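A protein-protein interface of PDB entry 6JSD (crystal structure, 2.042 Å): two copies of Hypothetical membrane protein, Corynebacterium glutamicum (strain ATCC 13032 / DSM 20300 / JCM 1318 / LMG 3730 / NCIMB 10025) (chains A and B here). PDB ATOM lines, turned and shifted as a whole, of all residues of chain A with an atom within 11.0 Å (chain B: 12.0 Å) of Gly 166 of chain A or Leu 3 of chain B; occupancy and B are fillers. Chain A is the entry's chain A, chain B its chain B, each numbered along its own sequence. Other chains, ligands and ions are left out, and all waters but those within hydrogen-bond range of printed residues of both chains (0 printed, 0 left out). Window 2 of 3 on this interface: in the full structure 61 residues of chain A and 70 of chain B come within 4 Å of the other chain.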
ATOM      1  N   ASN A  48      -2.843   4.971   5.302  1.00  0.00           N
ATOM      2  CA  ASN A  48      -1.766   5.348   4.395  1.00  0.00           C
ATOM      3  C   ASN A  48      -1.678   4.343   3.259  1.00  0.00           C
ATOM      4  O   ASN A  48      -0.586   3.964   2.818  1.00  0.00           O
ATOM      5  CB  ASN A  48      -0.435   5.454   5.140  1.00  0.00           C
ATOM      6  CG  ASN A  48      -0.178   4.259   6.043  1.00  0.00           C
ATOM      7  OD1 ASN A  48      -0.033   3.127   5.576  1.00  0.00           O
ATOM      8  ND2 ASN A  48      -0.126   4.507   7.349  1.00  0.00           N
ATOM      9  N   SER A  49      -2.831   3.901   2.762  1.00  0.00           N
ATOM     10  CA  SER A  49      -2.855   2.745   1.877  1.00  0.00           C
ATOM     11  C   SER A  49      -3.978   2.863   0.854  1.00  0.00           C
ATOM     12  O   SER A  49      -5.107   3.231   1.185  1.00  0.00           O
ATOM     13  CB  SER A  49      -3.015   1.460   2.707  1.00  0.00           C
ATOM     14  OG  SER A  49      -3.407   0.375   1.896  1.00  0.00           O
ATOM     15  N   GLY A  50      -3.670   2.526  -0.376  1.00  0.00           N
ATOM     16  CA  GLY A  50      -4.684   2.480  -1.407  1.00  0.00           C
ATOM     17  C   GLY A  50      -4.098   2.861  -2.747  1.00  0.00           C
ATOM     18  O   GLY A  50      -2.901   3.095  -2.887  1.00  0.00           O
ATOM     19  N   ALA A  51      -4.982   2.902  -3.739  1.00  0.00           N
ATOM     20  CA  ALA A  51      -4.628   3.267  -5.101  1.00  0.00           C
ATOM     21  C   ALA A  51      -5.785   4.044  -5.712  1.00  0.00           C
ATOM     22  O   ALA A  51      -6.954   3.820  -5.372  1.00  0.00           O
ATOM     23  CB  ALA A  51      -4.304   2.037  -5.955  1.00  0.00           C
ATOM     24  N   VAL A  52      -5.446   4.975  -6.603  1.00  0.00           N
ATOM     25  CA  VAL A  52      -6.427   5.829  -7.264  1.00  0.00           C
ATOM     26  C   VAL A  52      -6.005   6.012  -8.717  1.00  0.00           C
ATOM     27  O   VAL A  52      -4.856   6.367  -9.001  1.00  0.00           O
ATOM     28  CB  VAL A  52      -6.561   7.200  -6.573  1.00  0.00           C
ATOM     29  CG1 VAL A  52      -7.172   8.229  -7.540  1.00  0.00           C
ATOM     30  CG2 VAL A  52      -7.372   7.099  -5.284  1.00  0.00           C
ATOM     31  N   ASP A  53      -6.924   5.738  -9.637  1.00  0.00           N
ATOM     32  CA  ASP A  53      -6.724   6.035 -11.056  1.00  0.00           C
ATOM     33  C   ASP A  53      -7.365   7.396 -11.295  1.00  0.00           C
ATOM     34  O   ASP A  53      -8.592   7.514 -11.350  1.00  0.00           O
ATOM     35  CB  ASP A  53      -7.335   4.942 -11.927  1.00  0.00           C
ATOM     36  CG  ASP A  53      -7.079   5.146 -13.424  1.00  0.00           C
ATOM     37  OD1 ASP A  53      -6.772   6.279 -13.867  1.00  0.00           O
ATOM     38  OD2 ASP A  53      -7.195   4.150 -14.167  1.00  0.00           O
ATOM     39  N   ALA A  54      -6.532   8.440 -11.395  1.00  0.00           N
ATOM     40  CA  ALA A  54      -7.046   9.802 -11.507  1.00  0.00           C
ATOM     41  C   ALA A  54      -7.614  10.100 -12.890  1.00  0.00           C
ATOM     42  O   ALA A  54      -8.475  10.978 -13.018  1.00  0.00           O
ATOM     43  CB  ALA A  54      -5.949  10.811 -11.158  1.00  0.00           C
ATOM     44  N   GLU A  55      -7.159   9.386 -13.922  1.00  0.00           N
ATOM     45  CA  GLU A  55      -7.719   9.553 -15.262  1.00  0.00           C
ATOM     46  C   GLU A  55      -9.175   9.102 -15.315  1.00  0.00           C
ATOM     47  O   GLU A  55     -10.045   9.832 -15.802  1.00  0.00           O
ATOM     48  CB  GLU A  55      -6.882   8.773 -16.271  1.00  0.00           C
ATOM     49  CG  GLU A  55      -7.618   8.404 -17.542  1.00  0.00           C
ATOM     50  CD  GLU A  55      -7.350   9.376 -18.669  1.00  0.00           C
ATOM     51  OE1 GLU A  55      -6.349  10.118 -18.578  1.00  0.00           O
ATOM     52  OE2 GLU A  55      -8.136   9.396 -19.641  1.00  0.00           O
ATOM     53  N   ASN A  56      -9.460   7.901 -14.816  1.00  0.00           N
ATOM     54  CA  ASN A  56     -10.799   7.330 -14.870  1.00  0.00           C
ATOM     55  C   ASN A  56     -11.614   7.613 -13.619  1.00  0.00           C
ATOM     56  O   ASN A  56     -12.803   7.279 -13.585  1.00  0.00           O
ATOM     57  CB  ASN A  56     -10.710   5.821 -15.108  1.00  0.00           C
ATOM     58  CG  ASN A  56     -10.013   5.493 -16.409  1.00  0.00           C
ATOM     59  OD1 ASN A  56     -10.175   6.202 -17.399  1.00  0.00           O
ATOM     60  ND2 ASN A  56      -9.224   4.429 -16.413  1.00  0.00           N
ATOM     61  N   LYS A  57     -11.008   8.234 -12.609  1.00  0.00           N
ATOM     62  CA  LYS A  57     -11.677   8.565 -11.357  1.00  0.00           C
ATOM     63  C   LYS A  57     -12.234   7.306 -10.682  1.00  0.00           C
ATOM     64  O   LYS A  57     -13.396   7.254 -10.270  1.00  0.00           O
ATOM     65  CB  LYS A  57     -12.765   9.626 -11.576  1.00  0.00           C
ATOM     66  CG  LYS A  57     -12.210  11.019 -11.862  1.00  0.00           C
ATOM     67  CD  LYS A  57     -13.219  11.886 -12.601  1.00  0.00           C
ATOM     68  CE  LYS A  57     -12.614  13.226 -13.041  1.00  0.00           C
ATOM     69  NZ  LYS A  57     -12.593  14.250 -11.947  1.00  0.00           N
ATOM     70  N   THR A  58     -11.382   6.281 -10.579  1.00  0.00           N
ATOM     71  CA  THR A  58     -11.633   5.110  -9.747  1.00  0.00           C
ATOM     72  C   THR A  58     -10.549   4.998  -8.681  1.00  0.00           C
ATOM     73  O   THR A  58      -9.416   5.459  -8.872  1.00  0.00           O
ATOM     74  CB  THR A  58     -11.661   3.812 -10.567  1.00  0.00           C
ATOM     75  OG1 THR A  58     -10.326   3.310 -10.714  1.00  0.00           O
ATOM     76  CG2 THR A  58     -12.260   4.058 -11.936  1.00  0.00           C
ATOM     77  N   GLY A  59     -10.895   4.363  -7.564  1.00  0.00           N
ATOM     78  CA  GLY A  59      -9.942   4.247  -6.476  1.00  0.00           C
ATOM     79  C   GLY A  59     -10.449   3.355  -5.360  1.00  0.00           C
ATOM     80  O   GLY A  59     -11.621   2.969  -5.314  1.00  0.00           O
ATOM     81  N   SER A  60      -9.523   3.036  -4.456  1.00  0.00           N
ATOM     82  CA  SER A  60      -9.782   2.260  -3.243  1.00  0.00           C
ATOM     83  C   SER A  60      -8.847   2.790  -2.174  1.00  0.00           C
ATOM     84  O   SER A  60      -7.636   2.867  -2.399  1.00  0.00           O
ATOM     85  CB  SER A  60      -9.542   0.761  -3.453  1.00  0.00           C
ATOM     86  OG  SER A  60     -10.691   0.127  -3.974  1.00  0.00           O
ATOM     87  N   ILE A  61      -9.414   3.200  -1.049  1.00  0.00           N
ATOM     88  CA  ILE A  61      -8.684   3.792   0.060  1.00  0.00           C
ATOM     89  C   ILE A  61      -8.863   2.867   1.260  1.00  0.00           C
ATOM     90  O   ILE A  61     -10.001   2.583   1.654  1.00  0.00           O
ATOM     91  CB  ILE A  61      -9.219   5.192   0.398  1.00  0.00           C
ATOM     92  CG1 ILE A  61      -9.525   6.014  -0.880  1.00  0.00           C
ATOM     93  CG2 ILE A  61      -8.273   5.894   1.334  1.00  0.00           C
ATOM     94  CD1 ILE A  61      -8.345   6.294  -1.747  1.00  0.00           C
ATOM     95  N   ASN A  62      -7.755   2.428   1.853  1.00  0.00           N
ATOM     96  CA  ASN A  62      -7.782   1.499   2.979  1.00  0.00           C
ATOM     97  C   ASN A  62      -7.538   2.195   4.307  1.00  0.00           C
ATOM     98  O   ASN A  62      -6.772   3.156   4.388  1.00  0.00           O
ATOM     99  CB  ASN A  62      -6.737   0.405   2.802  1.00  0.00           C
ATOM    100  CG  ASN A  62      -7.099  -0.536   1.719  1.00  0.00           C
ATOM    101  OD1 ASN A  62      -8.108  -1.228   1.816  1.00  0.00           O
ATOM    102  ND2 ASN A  62      -6.302  -0.564   0.659  1.00  0.00           N
ATOM    103  N   PHE A  87     -14.426   3.640  -5.051  1.00  0.00           N
ATOM    104  CA  PHE A  87     -15.269   4.470  -5.894  1.00  0.00           C
ATOM    105  C   PHE A  87     -14.936   4.217  -7.351  1.00  0.00           C
ATOM    106  O   PHE A  87     -13.806   3.871  -7.710  1.00  0.00           O
ATOM    107  CB  PHE A  87     -15.160   5.977  -5.570  1.00  0.00           C
ATOM    108  CG  PHE A  87     -13.766   6.541  -5.682  1.00  0.00           C
ATOM    109  CD1 PHE A  87     -12.916   6.532  -4.586  1.00  0.00           C
ATOM    110  CD2 PHE A  87     -13.318   7.098  -6.876  1.00  0.00           C
ATOM    111  CE1 PHE A  87     -11.643   7.044  -4.672  1.00  0.00           C
ATOM    112  CE2 PHE A  87     -12.038   7.618  -6.977  1.00  0.00           C
ATOM    113  CZ  PHE A  87     -11.196   7.595  -5.871  1.00  0.00           C
ATOM    114  N   ASN A 124     -13.926  14.755  -5.798  1.00  0.00           N
ATOM    115  CA  ASN A 124     -12.910  15.539  -6.485  1.00  0.00           C
ATOM    116  C   ASN A 124     -11.652  14.693  -6.604  1.00  0.00           C
ATOM    117  O   ASN A 124     -11.230  14.064  -5.621  1.00  0.00           O
ATOM    118  CB  ASN A 124     -12.616  16.833  -5.720  1.00  0.00           C
ATOM    119  CG  ASN A 124     -13.798  17.779  -5.697  1.00  0.00           C
ATOM    120  OD1 ASN A 124     -14.734  17.591  -4.930  1.00  0.00           O
ATOM    121  ND2 ASN A 124     -13.762  18.804  -6.561  1.00  0.00           N
ATOM    122  N   VAL A 125     -11.069  14.642  -7.804  1.00  0.00           N
ATOM    123  CA  VAL A 125      -9.877  13.829  -8.023  1.00  0.00           C
ATOM    124  C   VAL A 125      -8.891  14.599  -8.887  1.00  0.00           C
ATOM    125  O   VAL A 125      -9.263  15.170  -9.918  1.00  0.00           O
ATOM    126  CB  VAL A 125     -10.214  12.454  -8.642  1.00  0.00           C
ATOM    127  CG1 VAL A 125      -8.952  11.615  -8.809  1.00  0.00           C
ATOM    128  CG2 VAL A 125     -11.207  11.687  -7.735  1.00  0.00           C
ATOM    129  N   SER A 126      -7.642  14.654  -8.434  1.00  0.00           N
ATOM    130  CA  SER A 126      -6.521  15.178  -9.206  1.00  0.00           C
ATOM    131  C   SER A 126      -5.348  14.225  -9.008  1.00  0.00           C
ATOM    132  O   SER A 126      -5.470  13.186  -8.352  1.00  0.00           O
ATOM    133  CB  SER A 126      -6.157  16.601  -8.774  1.00  0.00           C
ATOM    134  OG  SER A 126      -5.634  16.601  -7.455  1.00  0.00           O
ATOM    135  N   ALA A 127      -4.193  14.592  -9.556  1.00  0.00           N
ATOM    136  CA  ALA A 127      -3.000  13.770  -9.395  1.00  0.00           C
ATOM    137  C   ALA A 127      -2.434  13.831  -7.983  1.00  0.00           C
ATOM    138  O   ALA A 127      -1.612  12.985  -7.623  1.00  0.00           O
ATOM    139  CB  ALA A 127      -1.927  14.202 -10.388  1.00  0.00           C
ATOM    140  N   THR A 128      -2.846  14.806  -7.176  1.00  0.00           N
ATOM    141  CA  THR A 128      -2.308  14.948  -5.837  1.00  0.00           C
ATOM    142  C   THR A 128      -3.322  14.643  -4.744  1.00  0.00           C
ATOM    143  O   THR A 128      -2.922  14.528  -3.581  1.00  0.00           O
ATOM    144  CB  THR A 128      -1.763  16.368  -5.614  1.00  0.00           C
ATOM    145  OG1 THR A 128      -2.864  17.280  -5.506  1.00  0.00           O
ATOM    146  CG2 THR A 128      -0.839  16.804  -6.776  1.00  0.00           C
ATOM    147  N   GLU A 129      -4.611  14.508  -5.066  1.00  0.00           N
ATOM    148  CA  GLU A 129      -5.594  14.336  -3.998  1.00  0.00           C
ATOM    149  C   GLU A 129      -6.897  13.749  -4.536  1.00  0.00           C
ATOM    150  O   GLU A 129      -7.282  13.991  -5.681  1.00  0.00           O
ATOM    151  CB  GLU A 129      -5.881  15.670  -3.288  1.00  0.00           C
ATOM    152  CG  GLU A 129      -5.870  15.570  -1.756  1.00  0.00           C
ATOM    153  CD  GLU A 129      -6.178  16.883  -1.062  1.00  0.00           C
ATOM    154  OE1 GLU A 129      -7.324  17.059  -0.595  1.00  0.00           O
ATOM    155  OE2 GLU A 129      -5.271  17.738  -0.983  1.00  0.00           O
ATOM    156  N   ALA A 130      -7.558  12.956  -3.687  1.00  0.00           N
ATOM    157  CA  ALA A 130      -8.905  12.459  -3.945  1.00  0.00           C
ATOM    158  C   ALA A 130      -9.717  12.607  -2.667  1.00  0.00           C
ATOM    159  O   ALA A 130      -9.260  12.212  -1.588  1.00  0.00           O
ATOM    160  CB  ALA A 130      -8.897  10.992  -4.406  1.00  0.00           C
ATOM    161  N   PHE A 161     -14.247  11.431   3.059  1.00  0.00           N
ATOM    162  CA  PHE A 161     -12.843  11.054   3.096  1.00  0.00           C
ATOM    163  C   PHE A 161     -12.005  12.056   2.312  1.00  0.00           C
ATOM    164  O   PHE A 161     -12.503  12.783   1.446  1.00  0.00           O
ATOM    165  CB  PHE A 161     -12.625   9.643   2.515  1.00  0.00           C
ATOM    166  CG  PHE A 161     -12.560   9.611   1.010  1.00  0.00           C
ATOM    167  CD1 PHE A 161     -13.722   9.633   0.248  1.00  0.00           C
ATOM    168  CD2 PHE A 161     -11.337   9.579   0.350  1.00  0.00           C
ATOM    169  CE1 PHE A 161     -13.667   9.612  -1.137  1.00  0.00           C
ATOM    170  CE2 PHE A 161     -11.278   9.567  -1.046  1.00  0.00           C
ATOM    171  CZ  PHE A 161     -12.447   9.576  -1.780  1.00  0.00           C
ATOM    172  N   ALA A 163      -7.752  11.995   0.686  1.00  0.00           N
ATOM    173  CA  ALA A 163      -6.515  11.252   0.568  1.00  0.00           C
ATOM    174  C   ALA A 163      -5.537  12.027  -0.304  1.00  0.00           C
ATOM    175  O   ALA A 163      -5.916  12.566  -1.349  1.00  0.00           O
ATOM    176  CB  ALA A 163      -6.768   9.859  -0.014  1.00  0.00           C
ATOM    177  N   THR A 164      -4.286  12.090   0.139  1.00  0.00           N
ATOM    178  CA  THR A 164      -3.207  12.620  -0.680  1.00  0.00           C
ATOM    179  C   THR A 164      -2.558  11.479  -1.455  1.00  0.00           C
ATOM    180  O   THR A 164      -2.364  10.376  -0.925  1.00  0.00           O
ATOM    181  CB  THR A 164      -2.173  13.349   0.181  1.00  0.00           C
ATOM    182  OG1 THR A 164      -1.725  12.477   1.219  1.00  0.00           O
ATOM    183  CG2 THR A 164      -2.786  14.581   0.822  1.00  0.00           C
ATOM    184  N   LEU A 165      -2.237  11.749  -2.721  1.00  0.00           N
ATOM    185  CA  LEU A 165      -1.755  10.753  -3.662  1.00  0.00           C
ATOM    186  C   LEU A 165      -0.286  10.989  -3.988  1.00  0.00           C
ATOM    187  O   LEU A 165       0.243  12.089  -3.803  1.00  0.00           O
ATOM    188  CB  LEU A 165      -2.577  10.781  -4.958  1.00  0.00           C
ATOM    189  CG  LEU A 165      -4.094  10.663  -4.790  1.00  0.00           C
ATOM    190  CD1 LEU A 165      -4.820  10.685  -6.166  1.00  0.00           C
ATOM    191  CD2 LEU A 165      -4.478   9.420  -3.946  1.00  0.00           C
ATOM    192  N   GLY A 166       0.362   9.942  -4.494  1.00  0.00           N
ATOM    193  CA  GLY A 166       1.749  10.023  -4.926  1.00  0.00           C
ATOM    194  C   GLY A 166       2.008   9.437  -6.304  1.00  0.00           C
ATOM    195  O   GLY A 166       2.451   8.293  -6.433  1.00  0.00           O
ATOM    196  N   SER B   2      -1.700   4.772 -12.150  1.00  0.00           N
ATOM    197  CA  SER B   2      -2.328   4.454 -10.871  1.00  0.00           C
ATOM    198  C   SER B   2      -1.444   4.930  -9.721  1.00  0.00           C
ATOM    199  O   SER B   2      -0.286   4.529  -9.606  1.00  0.00           O
ATOM    200  CB  SER B   2      -2.601   2.955 -10.758  1.00  0.00           C
ATOM    201  OG  SER B   2      -3.295   2.659  -9.559  1.00  0.00           O
ATOM    202  N   LEU B   3      -2.007   5.785  -8.874  1.00  0.00           N
ATOM    203  CA  LEU B   3      -1.258   6.516  -7.861  1.00  0.00           C
ATOM    204  C   LEU B   3      -1.498   5.902  -6.489  1.00  0.00           C
ATOM    205  O   LEU B   3      -2.629   5.549  -6.151  1.00  0.00           O
ATOM    206  CB  LEU B   3      -1.669   7.997  -7.855  1.00  0.00           C
ATOM    207  CG  LEU B   3      -1.520   8.743  -9.194  1.00  0.00           C
ATOM    208  CD1 LEU B   3      -2.263  10.080  -9.189  1.00  0.00           C
ATOM    209  CD2 LEU B   3      -0.050   8.950  -9.560  1.00  0.00           C
ATOM    210  N   GLY B   4      -0.431   5.785  -5.695  1.00  0.00           N
ATOM    211  CA  GLY B   4      -0.585   5.314  -4.331  1.00  0.00           C
ATOM    212  C   GLY B   4      -1.077   6.399  -3.385  1.00  0.00           C
ATOM    213  O   GLY B   4      -0.943   7.603  -3.628  1.00  0.00           O
ATOM    214  N   VAL B   5      -1.667   5.960  -2.278  1.00  0.00           N
ATOM    215  CA  VAL B   5      -2.179   6.873  -1.263  1.00  0.00           C
ATOM    216  C   VAL B   5      -1.086   7.126  -0.228  1.00  0.00           C
ATOM    217  O   VAL B   5      -0.551   6.189   0.377  1.00  0.00           O
ATOM    218  CB  VAL B   5      -3.454   6.322  -0.606  1.00  0.00           C
ATOM    219  CG1 VAL B   5      -3.835   7.163   0.602  1.00  0.00           C
ATOM    220  CG2 VAL B   5      -4.596   6.309  -1.613  1.00  0.00           C
ATOM    221  N   THR B   6      -0.757   8.398  -0.029  1.00  0.00           N
ATOM    222  CA  THR B   6       0.258   8.784   0.942  1.00  0.00           C
ATOM    223  C   THR B   6      -0.321   8.813   2.351  1.00  0.00           C
ATOM    224  O   THR B   6       0.158   8.113   3.247  1.00  0.00           O
ATOM    225  CB  THR B   6       0.825  10.154   0.564  1.00  0.00           C
ATOM    226  OG1 THR B   6       1.493  10.044  -0.696  1.00  0.00           O
ATOM    227  CG2 THR B   6       1.799  10.655   1.621  1.00  0.00           C
ATOM    228  N   GLN B   7      -1.343   9.638   2.557  1.00  0.00           N
ATOM    229  CA  GLN B   7      -2.104   9.703   3.794  1.00  0.00           C
ATOM    230  C   GLN B   7      -3.571   9.791   3.427  1.00  0.00           C
ATOM    231  O   GLN B   7      -3.925  10.329   2.375  1.00  0.00           O
ATOM    232  CB  GLN B   7      -1.717  10.914   4.652  1.00  0.00           C
ATOM    233  CG  GLN B   7      -0.368  10.794   5.326  1.00  0.00           C
ATOM    234  CD  GLN B   7       0.158  12.135   5.791  1.00  0.00           C
ATOM    235  OE1 GLN B   7      -0.403  13.180   5.457  1.00  0.00           O
ATOM    236  NE2 GLN B   7       1.245  12.115   6.561  1.00  0.00           N
ATOM    237  N   ALA B   8      -4.425   9.252   4.292  1.00  0.00           N
ATOM    238  CA  ALA B   8      -5.858   9.358   4.073  1.00  0.00           C
ATOM    239  C   ALA B   8      -6.577   9.434   5.410  1.00  0.00           C
ATOM    240  O   ALA B   8      -6.077   8.969   6.438  1.00  0.00           O
ATOM    241  CB  ALA B   8      -6.403   8.190   3.258  1.00  0.00           C
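The backbone carbonyl oxygen of Thr 164 of chain A lies within hydrogen-bond range of the backbone NH of Thr 6 of chain B.
The backbone carbonyl oxygen of Gly 4 of chain B lies within hydrogen-bond range of the backbone NH of Gly 166 of chain A (2.8 Å).
The backbone carbonyl oxygen (O) of Asn 48 of chain A lies close to the backbone carbonyl oxygen (O) of Val 5 of chain B, at 3.3 Å.
The backbone carbonyl oxygen (O) of Val 52 of chain A sits at hydrogen-bond distance from the backbone NH (N) of Leu 3 of chain B (2.9 Å).
O of Gly 50 of chain A is in hydrogen-bond range of N of Val 5 of chain B (3.2 Å).
N of Thr 164 of chain A is in hydrogen-bond range of O of Gln 7 of chain B (2.9 Å).
The backbone carbonyl oxygen (O) of Thr 128 of chain A lies within hydrogen-bond range of the backbone NH (N) of Leu 165 of chain A, at 3.0 Å.
The backbone NH (N) of Ser 60 of chain A is in hydrogen-bond range of the backbone carbonyl oxygen (O) of Ala 51 of chain A, 2.8 Å away.
The backbone carbonyl oxygen of Ser 49 of chain A sits at hydrogen-bond distance from the backbone NH of Asn 62 of chain A, at 2.8 Å.
The backbone carbonyl oxygen of Ala 130 of chain A lies within hydrogen-bond range of the backbone NH of Ala 163 of chain A (2.7 Å).
Among the printed residues, merely in contact across the chains: Asn 48 of chain A with Thr 6 of chain B (3.3 Å), Ser 49 of chain A with Val 5 of chain B (3.8 Å), Gly 50 of chain A with Gly 4 of chain B (3.5 Å), Ala 51 of chain A with Ser 2 of chain B (3.8 Å), Ala 51 of chain A with Leu 3 of chain B (3.2 Å), Val 52 of chain A with Ser 2 of chain B (3.7 Å), Ile 61 of chain A with Val 5 of chain B (3.8 Å), Ile 61 of chain A with Ala 8 of chain B (3.5 Å), Ala 127 of chain A with Leu 3 of chain B (3.4 Å), Ala 163 of chain A with Gln 7 of chain B (3.3 Å), Ala 163 of chain A with Ala 8 of chain B (3.7 Å), Thr 164 of chain A with Val 5 of chain B (3.5 Å), Leu 165 of chain A with Gly 4 of chain B (3.3 Å), Leu 165 of chain A with Val 5 of chain B (3.9 Å), Leu 165 of chain A with Thr 6 of chain B (3.9 Å), Gly 166 of chain A with Leu 3 of chain B (3.9 Å) and Gly 166 of chain A with Thr 6 of chain B (3.96 Å).
Printed residues of chain B within 4 Å of Ser 49 of chain A: Val 5 (3.8 Å).
Gly 50 of chain A touches just these residues of chain B: Gly 4 (3.5 Å) and Val 5 (3.2 Å).
Of chain B, only Ser 2 and Leu 3 come within 4 Å of Ala 51 of chain A.
Val 52 of chain A touches two residues of chain B.
No residue of chain B comes within 4 Å of Ala 54 of chain A.
Gly 59 of chain A touches none of the printed residues of chain B.
Of the printed residues of chain B, Ile 61 of chain A touches Val 5 (3.8 Å) and Ala 8 (3.5 Å).
Of chain B, only Leu 3 (3.4 Å) comes within 4 Å of Ala 127 of chain A.
Printed residues of chain B within 4 Å of Thr 164 of chain A: Val 5, Thr 6 and Gln 7.
Gly 166 of chain A touches three residues of chain B.
Printed residues of chain A within 4 Å of Leu 3 of chain B: Ala 51, Val 52, Ala 127 and Gly 166.
Of chain A, only Gly 50 (3.5 Å), Leu 165 (3.3 Å) and Gly 166 (2.8 Å) come within 4 Å of Gly 4 of chain B.
The nearest residue of chain B that does not touch Gly 166 of chain A is Val 5 of chain B (5.0 Å).
The nearest printed residue of chain A that does not touch Val 5 of chain B is Ala 163 of chain A (4.03 Å).
Hydrophobic or aromatic side chains of chain A within 4 Å of the printed part of chain B: Ala 51, Ile 61, Ala 163 and Leu 165.
Hydrophobic or aromatic side chains of chain B within 4 Å of the printed part of chain A: Leu 3, Val 5 and Ala 8.
No position is printed for both chains.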
